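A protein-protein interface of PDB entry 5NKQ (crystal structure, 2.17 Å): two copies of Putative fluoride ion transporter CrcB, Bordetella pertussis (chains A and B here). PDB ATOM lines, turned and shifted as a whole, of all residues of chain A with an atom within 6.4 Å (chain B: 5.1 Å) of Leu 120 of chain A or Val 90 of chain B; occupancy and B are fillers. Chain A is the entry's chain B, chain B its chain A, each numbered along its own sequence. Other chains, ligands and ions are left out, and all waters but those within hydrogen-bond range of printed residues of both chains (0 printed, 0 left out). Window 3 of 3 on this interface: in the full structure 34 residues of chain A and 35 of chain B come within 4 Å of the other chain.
No position is printed for both chains. Of the 8 pairs that touch across the chains among the printed residues, none has its exchanged pair printed and touching as well.
Of the 10 printed residues of chain B, 4 touch a printed residue of chain A. Printed residues of chain A that touch a printed residue of chain B: Ile 50, Ser 112, Leu 113, Thr 116 and Leu 120. Hydrophobic or aromatic side chains of chain A that line the printed part of chain B: Ile 50, Leu 113 and Leu 120. Among the printed residues, 8 pairs touch across the chains.
OG of Ser 86 of chain B lies within hydrogen-bond range of OG1 of Thr 116 of chain A. The side-chain hydroxyl of Ser 86 of chain B lies within hydrogen-bond range of the backbone carbonyl oxygen of Ser 112 of chain A (3.0 Å).
Printed residues of chain B within 4 Å of Ile 50 of chain A: Ala 87. Printed residues of chain B within 4 Å of Ser 112 of chain A: Ser 86 (3.0 Å). Printed residues of chain B within 4 Å of Leu 113 of chain A: Ser 86 (3.6 Å), Thr 89 (3.8 Å) and Val 90 (3.8 Å). Of chain B, only Val 90 (3.8 Å) comes within 4 Å of Leu 120 of chain A. Arg 124 of chain A touches none of the printed residues of chain B. Leu 125 of chain A touches none of the printed residues of chain B. Of the printed residues of chain A, Ser 86 of chain B touches Ser 112, Leu 113 and Thr 116. Of the printed residues of chain A, Ala 87 of chain B touches Ile 50 (3.7 Å). Of chain A, only Leu 113, Thr 116 and Leu 120 come within 4 Å of Val 90 of chain B. The nearest printed residue of chain B that does not touch Leu 120 of chain A is Asp 91 of chain B (6.5 Å).
O of Phe 85 of chain B is in hydrogen-bond range of OG1 of Thr 89 of chain B, at 2.9 Å. SG of Cys 94 of chain B is in hydrogen-bond range of O of Val 90 of chain B (3.7 Å). The backbone carbonyl oxygen of Ser 112 of chain A sits at hydrogen-bond distance from the side-chain hydroxyl of Thr 116 of chain A, 3.0 Å away.
Among the printed residues, merely in contact across the chains: Ile 50 of chain A with Ala 87 of chain B (3.7 Å), Leu 113 of chain A with Ser 86 of chain B (3.6 Å), Leu 113 of chain A with Thr 89 of chain B (3.8 Å), Leu 113 of chain A with Val 90 of chain B (3.8 Å), Thr 116 of chain A with Val 90 of chain B (3.8 Å) and Leu 120 of chain A with Val 90 of chain B (3.8 Å).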
ATOM      1  N   TYR A  48      20.032   3.828   3.235  1.00  0.00           N
ATOM      2  CA  TYR A  48      20.301   2.929   4.353  1.00  0.00           C
ATOM      3  C   TYR A  48      21.720   2.379   4.288  1.00  0.00           C
ATOM      4  O   TYR A  48      22.411   2.306   5.310  1.00  0.00           O
ATOM      5  CB  TYR A  48      19.284   1.789   4.361  1.00  0.00           C
ATOM      6  CG  TYR A  48      19.551   0.724   5.401  1.00  0.00           C
ATOM      7  CD1 TYR A  48      19.117   0.881   6.712  1.00  0.00           C
ATOM      8  CD2 TYR A  48      20.228  -0.443   5.071  1.00  0.00           C
ATOM      9  CE1 TYR A  48      19.356  -0.093   7.664  1.00  0.00           C
ATOM     10  CE2 TYR A  48      20.473  -1.419   6.016  1.00  0.00           C
ATOM     11  CZ  TYR A  48      20.035  -1.240   7.310  1.00  0.00           C
ATOM     12  OH  TYR A  48      20.277  -2.211   8.252  1.00  0.00           O
ATOM     13  N   ILE A  50      24.420   3.615   2.946  1.00  0.00           N
ATOM     14  CA  ILE A  50      25.489   4.567   3.231  1.00  0.00           C
ATOM     15  C   ILE A  50      25.590   4.819   4.729  1.00  0.00           C
ATOM     16  O   ILE A  50      26.679   5.095   5.246  1.00  0.00           O
ATOM     17  CB  ILE A  50      25.298   5.874   2.436  1.00  0.00           C
ATOM     18  CG1 ILE A  50      26.606   6.669   2.411  1.00  0.00           C
ATOM     19  CG2 ILE A  50      24.178   6.720   3.020  1.00  0.00           C
ATOM     20  CD1 ILE A  50      26.571   7.880   1.509  1.00  0.00           C
ATOM     21  N   GLY A  51      24.474   4.713   5.455  1.00  0.00           N
ATOM     22  CA  GLY A  51      24.549   4.758   6.905  1.00  0.00           C
ATOM     23  C   GLY A  51      25.292   3.564   7.470  1.00  0.00           C
ATOM     24  O   GLY A  51      26.021   3.684   8.458  1.00  0.00           O
ATOM     25  N   VAL A  52      25.124   2.398   6.844  1.00  0.00           N
ATOM     26  CA  VAL A  52      25.883   1.217   7.245  1.00  0.00           C
ATOM     27  C   VAL A  52      27.362   1.407   6.931  1.00  0.00           C
ATOM     28  O   VAL A  52      28.231   1.124   7.765  1.00  0.00           O
ATOM     29  CB  VAL A  52      25.317  -0.039   6.558  1.00  0.00           C
ATOM     30  CG1 VAL A  52      26.199  -1.246   6.840  1.00  0.00           C
ATOM     31  CG2 VAL A  52      23.890  -0.297   7.015  1.00  0.00           C
ATOM     32  N   VAL A  54      29.121   4.209   6.497  1.00  0.00           N
ATOM     33  CA  VAL A  54      29.747   5.242   7.319  1.00  0.00           C
ATOM     34  C   VAL A  54      30.116   4.685   8.688  1.00  0.00           C
ATOM     35  O   VAL A  54      31.213   4.938   9.205  1.00  0.00           O
ATOM     36  CB  VAL A  54      28.822   6.470   7.431  1.00  0.00           C
ATOM     37  CG1 VAL A  54      29.251   7.361   8.586  1.00  0.00           C
ATOM     38  CG2 VAL A  54      28.828   7.255   6.127  1.00  0.00           C
ATOM     39  N   ALA A  55      29.218   3.904   9.292  1.00  0.00           N
ATOM     40  CA  ALA A  55      29.522   3.308  10.587  1.00  0.00           C
ATOM     41  C   ALA A  55      30.562   2.201  10.467  1.00  0.00           C
ATOM     42  O   ALA A  55      31.350   1.991  11.396  1.00  0.00           O
ATOM     43  CB  ALA A  55      28.245   2.777  11.234  1.00  0.00           C
ATOM     44  N   SER A 112      14.973   8.917   3.094  1.00  0.00           N
ATOM     45  CA  SER A 112      16.390   8.586   2.978  1.00  0.00           C
ATOM     46  C   SER A 112      17.162   9.012   4.220  1.00  0.00           C
ATOM     47  O   SER A 112      18.088   8.315   4.650  1.00  0.00           O
ATOM     48  CB  SER A 112      16.983   9.236   1.728  1.00  0.00           C
ATOM     49  OG  SER A 112      18.356   8.917   1.590  1.00  0.00           O
ATOM     50  N   LEU A 113      16.799  10.157   4.809  1.00  0.00           N
ATOM     51  CA  LEU A 113      17.451  10.590   6.041  1.00  0.00           C
ATOM     52  C   LEU A 113      17.189   9.607   7.175  1.00  0.00           C
ATOM     53  O   LEU A 113      18.059   9.381   8.025  1.00  0.00           O
ATOM     54  CB  LEU A 113      16.975  11.988   6.432  1.00  0.00           C
ATOM     55  CG  LEU A 113      17.293  13.140   5.479  1.00  0.00           C
ATOM     56  CD1 LEU A 113      16.797  14.456   6.063  1.00  0.00           C
ATOM     57  CD2 LEU A 113      18.782  13.204   5.181  1.00  0.00           C
ATOM     58  N   ALA A 114      15.992   9.016   7.206  1.00  0.00           N
ATOM     59  CA  ALA A 114      15.679   8.040   8.242  1.00  0.00           C
ATOM     60  C   ALA A 114      16.419   6.729   8.006  1.00  0.00           C
ATOM     61  O   ALA A 114      16.888   6.095   8.959  1.00  0.00           O
ATOM     62  CB  ALA A 114      14.170   7.802   8.305  1.00  0.00           C
ATOM     63  N   MET A 115      16.534   6.306   6.745  1.00  0.00           N
ATOM     64  CA  MET A 115      17.247   5.067   6.450  1.00  0.00           C
ATOM     65  C   MET A 115      18.732   5.197   6.766  1.00  0.00           C
ATOM     66  O   MET A 115      19.364   4.232   7.207  1.00  0.00           O
ATOM     67  CB  MET A 115      17.038   4.669   4.989  1.00  0.00           C
ATOM     68  CG  MET A 115      15.590   4.384   4.615  1.00  0.00           C
ATOM     69  SD  MET A 115      14.816   3.116   5.640  1.00  0.00           S
ATOM     70  CE  MET A 115      15.781   1.674   5.204  1.00  0.00           C
ATOM     71  N   THR A 116      19.306   6.383   6.546  1.00  0.00           N
ATOM     72  CA  THR A 116      20.702   6.602   6.913  1.00  0.00           C
ATOM     73  C   THR A 116      20.890   6.509   8.422  1.00  0.00           C
ATOM     74  O   THR A 116      21.843   5.882   8.898  1.00  0.00           O
ATOM     75  CB  THR A 116      21.179   7.959   6.394  1.00  0.00           C
ATOM     76  OG1 THR A 116      21.048   7.999   4.967  1.00  0.00           O
ATOM     77  CG2 THR A 116      22.636   8.191   6.767  1.00  0.00           C
ATOM     78  N   GLY A 117      19.988   7.125   9.190  1.00  0.00           N
ATOM     79  CA  GLY A 117      20.031   6.966  10.635  1.00  0.00           C
ATOM     80  C   GLY A 117      19.846   5.523  11.062  1.00  0.00           C
ATOM     81  O   GLY A 117      20.494   5.054  12.001  1.00  0.00           O
ATOM     82  N   LEU A 118      18.956   4.799  10.379  1.00  0.00           N
ATOM     83  CA  LEU A 118      18.797   3.374  10.646  1.00  0.00           C
ATOM     84  C   LEU A 118      20.038   2.591  10.245  1.00  0.00           C
ATOM     85  O   LEU A 118      20.386   1.604  10.904  1.00  0.00           O
ATOM     86  CB  LEU A 118      17.569   2.833   9.916  1.00  0.00           C
ATOM     87  CG  LEU A 118      16.202   3.204  10.498  1.00  0.00           C
ATOM     88  CD1 LEU A 118      15.082   2.650   9.628  1.00  0.00           C
ATOM     89  CD2 LEU A 118      16.074   2.695  11.926  1.00  0.00           C
ATOM     90  N   GLY A 119      20.715   3.007   9.173  1.00  0.00           N
ATOM     91  CA  GLY A 119      21.949   2.343   8.790  1.00  0.00           C
ATOM     92  C   GLY A 119      23.060   2.564   9.796  1.00  0.00           C
ATOM     93  O   GLY A 119      23.889   1.678  10.025  1.00  0.00           O
ATOM     94  N   LEU A 120      23.094   3.747  10.413  1.00  0.00           N
ATOM     95  CA  LEU A 120      24.070   4.004  11.466  1.00  0.00           C
ATOM     96  C   LEU A 120      23.754   3.190  12.715  1.00  0.00           C
ATOM     97  O   LEU A 120      24.664   2.674  13.376  1.00  0.00           O
ATOM     98  CB  LEU A 120      24.106   5.496  11.795  1.00  0.00           C
ATOM     99  CG  LEU A 120      24.576   6.459  10.700  1.00  0.00           C
ATOM    100  CD1 LEU A 120      24.236   7.892  11.073  1.00  0.00           C
ATOM    101  CD2 LEU A 120      26.070   6.311  10.464  1.00  0.00           C
ATOM    102  N   ALA A 121      22.469   3.055  13.045  1.00  0.00           N
ATOM    103  CA  ALA A 121      22.061   2.389  14.277  1.00  0.00           C
ATOM    104  C   ALA A 121      22.216   0.876  14.207  1.00  0.00           C
ATOM    105  O   ALA A 121      22.524   0.247  15.226  1.00  0.00           O
ATOM    106  CB  ALA A 121      20.610   2.747  14.610  1.00  0.00           C
ATOM    107  N   THR A 122      22.006   0.271  13.035  1.00  0.00           N
ATOM    108  CA  THR A 122      22.120  -1.182  12.930  1.00  0.00           C
ATOM    109  C   THR A 122      23.553  -1.651  13.144  1.00  0.00           C
ATOM    110  O   THR A 122      23.774  -2.741  13.685  1.00  0.00           O
ATOM    111  CB  THR A 122      21.605  -1.661  11.573  1.00  0.00           C
ATOM    112  OG1 THR A 122      22.200  -0.880  10.528  1.00  0.00           O
ATOM    113  CG2 THR A 122      20.089  -1.537  11.502  1.00  0.00           C
ATOM    114  N   VAL A 123      24.537  -0.852  12.730  1.00  0.00           N
ATOM    115  CA  VAL A 123      25.929  -1.229  12.941  1.00  0.00           C
ATOM    116  C   VAL A 123      26.327  -1.003  14.393  1.00  0.00           C
ATOM    117  O   VAL A 123      27.065  -1.803  14.979  1.00  0.00           O
ATOM    118  CB  VAL A 123      26.842  -0.455  11.971  1.00  0.00           C
ATOM    119  CG1 VAL A 123      28.305  -0.762  12.255  1.00  0.00           C
ATOM    120  CG2 VAL A 123      26.497  -0.795  10.531  1.00  0.00           C
ATOM    121  N   ARG A 124      25.832   0.075  15.003  1.00  0.00           N
ATOM    122  CA  ARG A 124      26.148   0.373  16.395  1.00  0.00           C
ATOM    123  C   ARG A 124      25.473  -0.581  17.373  1.00  0.00           C
ATOM    124  O   ARG A 124      25.851  -0.602  18.549  1.00  0.00           O
ATOM    125  CB  ARG A 124      25.766   1.819  16.710  1.00  0.00           C
ATOM    126  CG  ARG A 124      26.667   2.837  16.027  1.00  0.00           C
ATOM    127  CD  ARG A 124      26.017   4.204  15.927  1.00  0.00           C
ATOM    128  NE  ARG A 124      26.883   5.147  15.226  1.00  0.00           N
ATOM    129  CZ  ARG A 124      26.498   6.344  14.799  1.00  0.00           C
ATOM    130  NH1 ARG A 124      25.252   6.751  14.997  1.00  0.00           N
ATOM    131  NH2 ARG A 124      27.358   7.132  14.170  1.00  0.00           N
ATOM    132  N   LEU A 125      24.495  -1.367  16.922  1.00  0.00           N
ATOM    133  CA  LEU A 125      23.883  -2.385  17.764  1.00  0.00           C
ATOM    134  C   LEU A 125      24.589  -3.730  17.662  1.00  0.00           C
ATOM    135  O   LEU A 125      24.666  -4.459  18.657  1.00  0.00           O
ATOM    136  CB  LEU A 125      22.405  -2.559  17.401  1.00  0.00           C
ATOM    137  CG  LEU A 125      21.372  -1.831  18.265  1.00  0.00           C
ATOM    138  CD1 LEU A 125      21.639  -0.336  18.296  1.00  0.00           C
ATOM    139  CD2 LEU A 125      19.966  -2.119  17.760  1.00  0.00           C
ATOM    140  N   PHE B  85      24.186  12.905  -0.440  1.00  0.00           N
ATOM    141  CA  PHE B  85      23.421  14.009   0.129  1.00  0.00           C
ATOM    142  C   PHE B  85      22.816  13.625   1.473  1.00  0.00           C
ATOM    143  O   PHE B  85      22.792  14.435   2.407  1.00  0.00           O
ATOM    144  CB  PHE B  85      22.328  14.445  -0.850  1.00  0.00           C
ATOM    145  CG  PHE B  85      21.194  15.191  -0.202  1.00  0.00           C
ATOM    146  CD1 PHE B  85      21.320  16.534   0.109  1.00  0.00           C
ATOM    147  CD2 PHE B  85      20.001  14.549   0.089  1.00  0.00           C
ATOM    148  CE1 PHE B  85      20.281  17.222   0.705  1.00  0.00           C
ATOM    149  CE2 PHE B  85      18.958  15.233   0.685  1.00  0.00           C
ATOM    150  CZ  PHE B  85      19.098  16.571   0.993  1.00  0.00           C
ATOM    151  N   SER B  86      22.333  12.387   1.593  1.00  0.00           N
ATOM    152  CA  SER B  86      21.704  11.952   2.835  1.00  0.00           C
ATOM    153  C   SER B  86      22.720  11.850   3.967  1.00  0.00           C
ATOM    154  O   SER B  86      22.442  12.271   5.096  1.00  0.00           O
ATOM    155  CB  SER B  86      20.999  10.612   2.622  1.00  0.00           C
ATOM    156  OG  SER B  86      20.269  10.227   3.773  1.00  0.00           O
ATOM    157  N   ALA B  87      23.904  11.298   3.686  1.00  0.00           N
ATOM    158  CA  ALA B  87      24.915  11.153   4.728  1.00  0.00           C
ATOM    159  C   ALA B  87      25.466  12.505   5.160  1.00  0.00           C
ATOM    160  O   ALA B  87      25.733  12.721   6.348  1.00  0.00           O
ATOM    161  CB  ALA B  87      26.043  10.243   4.242  1.00  0.00           C
ATOM    162  N   GLU B  88      25.649  13.427   4.211  1.00  0.00           N
ATOM    163  CA  GLU B  88      26.105  14.768   4.562  1.00  0.00           C
ATOM    164  C   GLU B  88      25.079  15.485   5.431  1.00  0.00           C
ATOM    165  O   GLU B  88      25.436  16.134   6.422  1.00  0.00           O
ATOM    166  CB  GLU B  88      26.393  15.575   3.296  1.00  0.00           C
ATOM    167  CG  GLU B  88      27.566  15.057   2.478  1.00  0.00           C
ATOM    168  CD  GLU B  88      27.577  15.602   1.060  1.00  0.00           C
ATOM    169  OE1 GLU B  88      28.671  15.697   0.466  1.00  0.00           O
ATOM    170  OE2 GLU B  88      26.491  15.934   0.539  1.00  0.00           O
ATOM    171  N   THR B  89      23.796  15.373   5.078  1.00  0.00           N
ATOM    172  CA  THR B  89      22.750  16.020   5.863  1.00  0.00           C
ATOM    173  C   THR B  89      22.642  15.406   7.254  1.00  0.00           C
ATOM    174  O   THR B  89      22.496  16.128   8.248  1.00  0.00           O
ATOM    175  CB  THR B  89      21.412  15.928   5.127  1.00  0.00           C
ATOM    176  OG1 THR B  89      21.527  16.567   3.849  1.00  0.00           O
ATOM    177  CG2 THR B  89      20.308  16.604   5.926  1.00  0.00           C
ATOM    178  N   VAL B  90      22.719  14.076   7.345  1.00  0.00           N
ATOM    179  CA  VAL B  90      22.659  13.413   8.645  1.00  0.00           C
ATOM    180  C   VAL B  90      23.837  13.838   9.516  1.00  0.00           C
ATOM    181  O   VAL B  90      23.690  14.034  10.730  1.00  0.00           O
ATOM    182  CB  VAL B  90      22.603  11.884   8.461  1.00  0.00           C
ATOM    183  CG1 VAL B  90      22.908  11.168   9.769  1.00  0.00           C
ATOM    184  CG2 VAL B  90      21.234  11.469   7.941  1.00  0.00           C
ATOM    185  N   ASP B  91      25.017  14.006   8.912  1.00  0.00           N
ATOM    186  CA  ASP B  91      26.170  14.462   9.682  1.00  0.00           C
ATOM    187  C   ASP B  91      25.978  15.886  10.188  1.00  0.00           C
ATOM    188  O   ASP B  91      26.503  16.240  11.250  1.00  0.00           O
ATOM    189  CB  ASP B  91      27.445  14.368   8.844  1.00  0.00           C
ATOM    190  CG  ASP B  91      28.699  14.592   9.672  1.00  0.00           C
ATOM    191  OD1 ASP B  91      29.091  13.669  10.417  1.00  0.00           O
ATOM    192  OD2 ASP B  91      29.288  15.691   9.588  1.00  0.00           O
ATOM    193  N   MET B  92      25.240  16.716   9.448  1.00  0.00           N
ATOM    194  CA  MET B  92      24.914  18.045   9.950  1.00  0.00           C
ATOM    195  C   MET B  92      23.957  17.972  11.132  1.00  0.00           C
ATOM    196  O   MET B  92      24.048  18.791  12.054  1.00  0.00           O
ATOM    197  CB  MET B  92      24.311  18.901   8.834  1.00  0.00           C
ATOM    198  CG  MET B  92      25.242  19.158   7.660  1.00  0.00           C
ATOM    199  SD  MET B  92      24.450  20.121   6.356  1.00  0.00           S
ATOM    200  CE  MET B  92      25.760  20.198   5.140  1.00  0.00           C
ATOM    201  N   LEU B  93      23.046  16.997  11.129  1.00  0.00           N
ATOM    202  CA  LEU B  93      22.066  16.894  12.207  1.00  0.00           C
ATOM    203  C   LEU B  93      22.719  16.467  13.515  1.00  0.00           C
ATOM    204  O   LEU B  93      22.388  16.999  14.581  1.00  0.00           O
ATOM    205  CB  LEU B  93      20.956  15.920  11.813  1.00  0.00           C
ATOM    206  CG  LEU B  93      20.040  16.371  10.675  1.00  0.00           C
ATOM    207  CD1 LEU B  93      19.073  15.265  10.294  1.00  0.00           C
ATOM    208  CD2 LEU B  93      19.287  17.633  11.066  1.00  0.00           C
ATOM    209  N   CYS B  94      23.644  15.506  13.460  1.00  0.00           N
ATOM    210  CA  CYS B  94      24.317  15.067  14.676  1.00  0.00           C
ATOM    211  C   CYS B  94      25.285  16.115  15.210  1.00  0.00           C
ATOM    212  O   CYS B  94      25.650  16.060  16.389  1.00  0.00           O
ATOM    213  CB  CYS B  94      25.050  13.747  14.432  1.00  0.00           C
ATOM    214  SG  CYS B  94      26.395  13.838  13.236  1.00  0.00           S
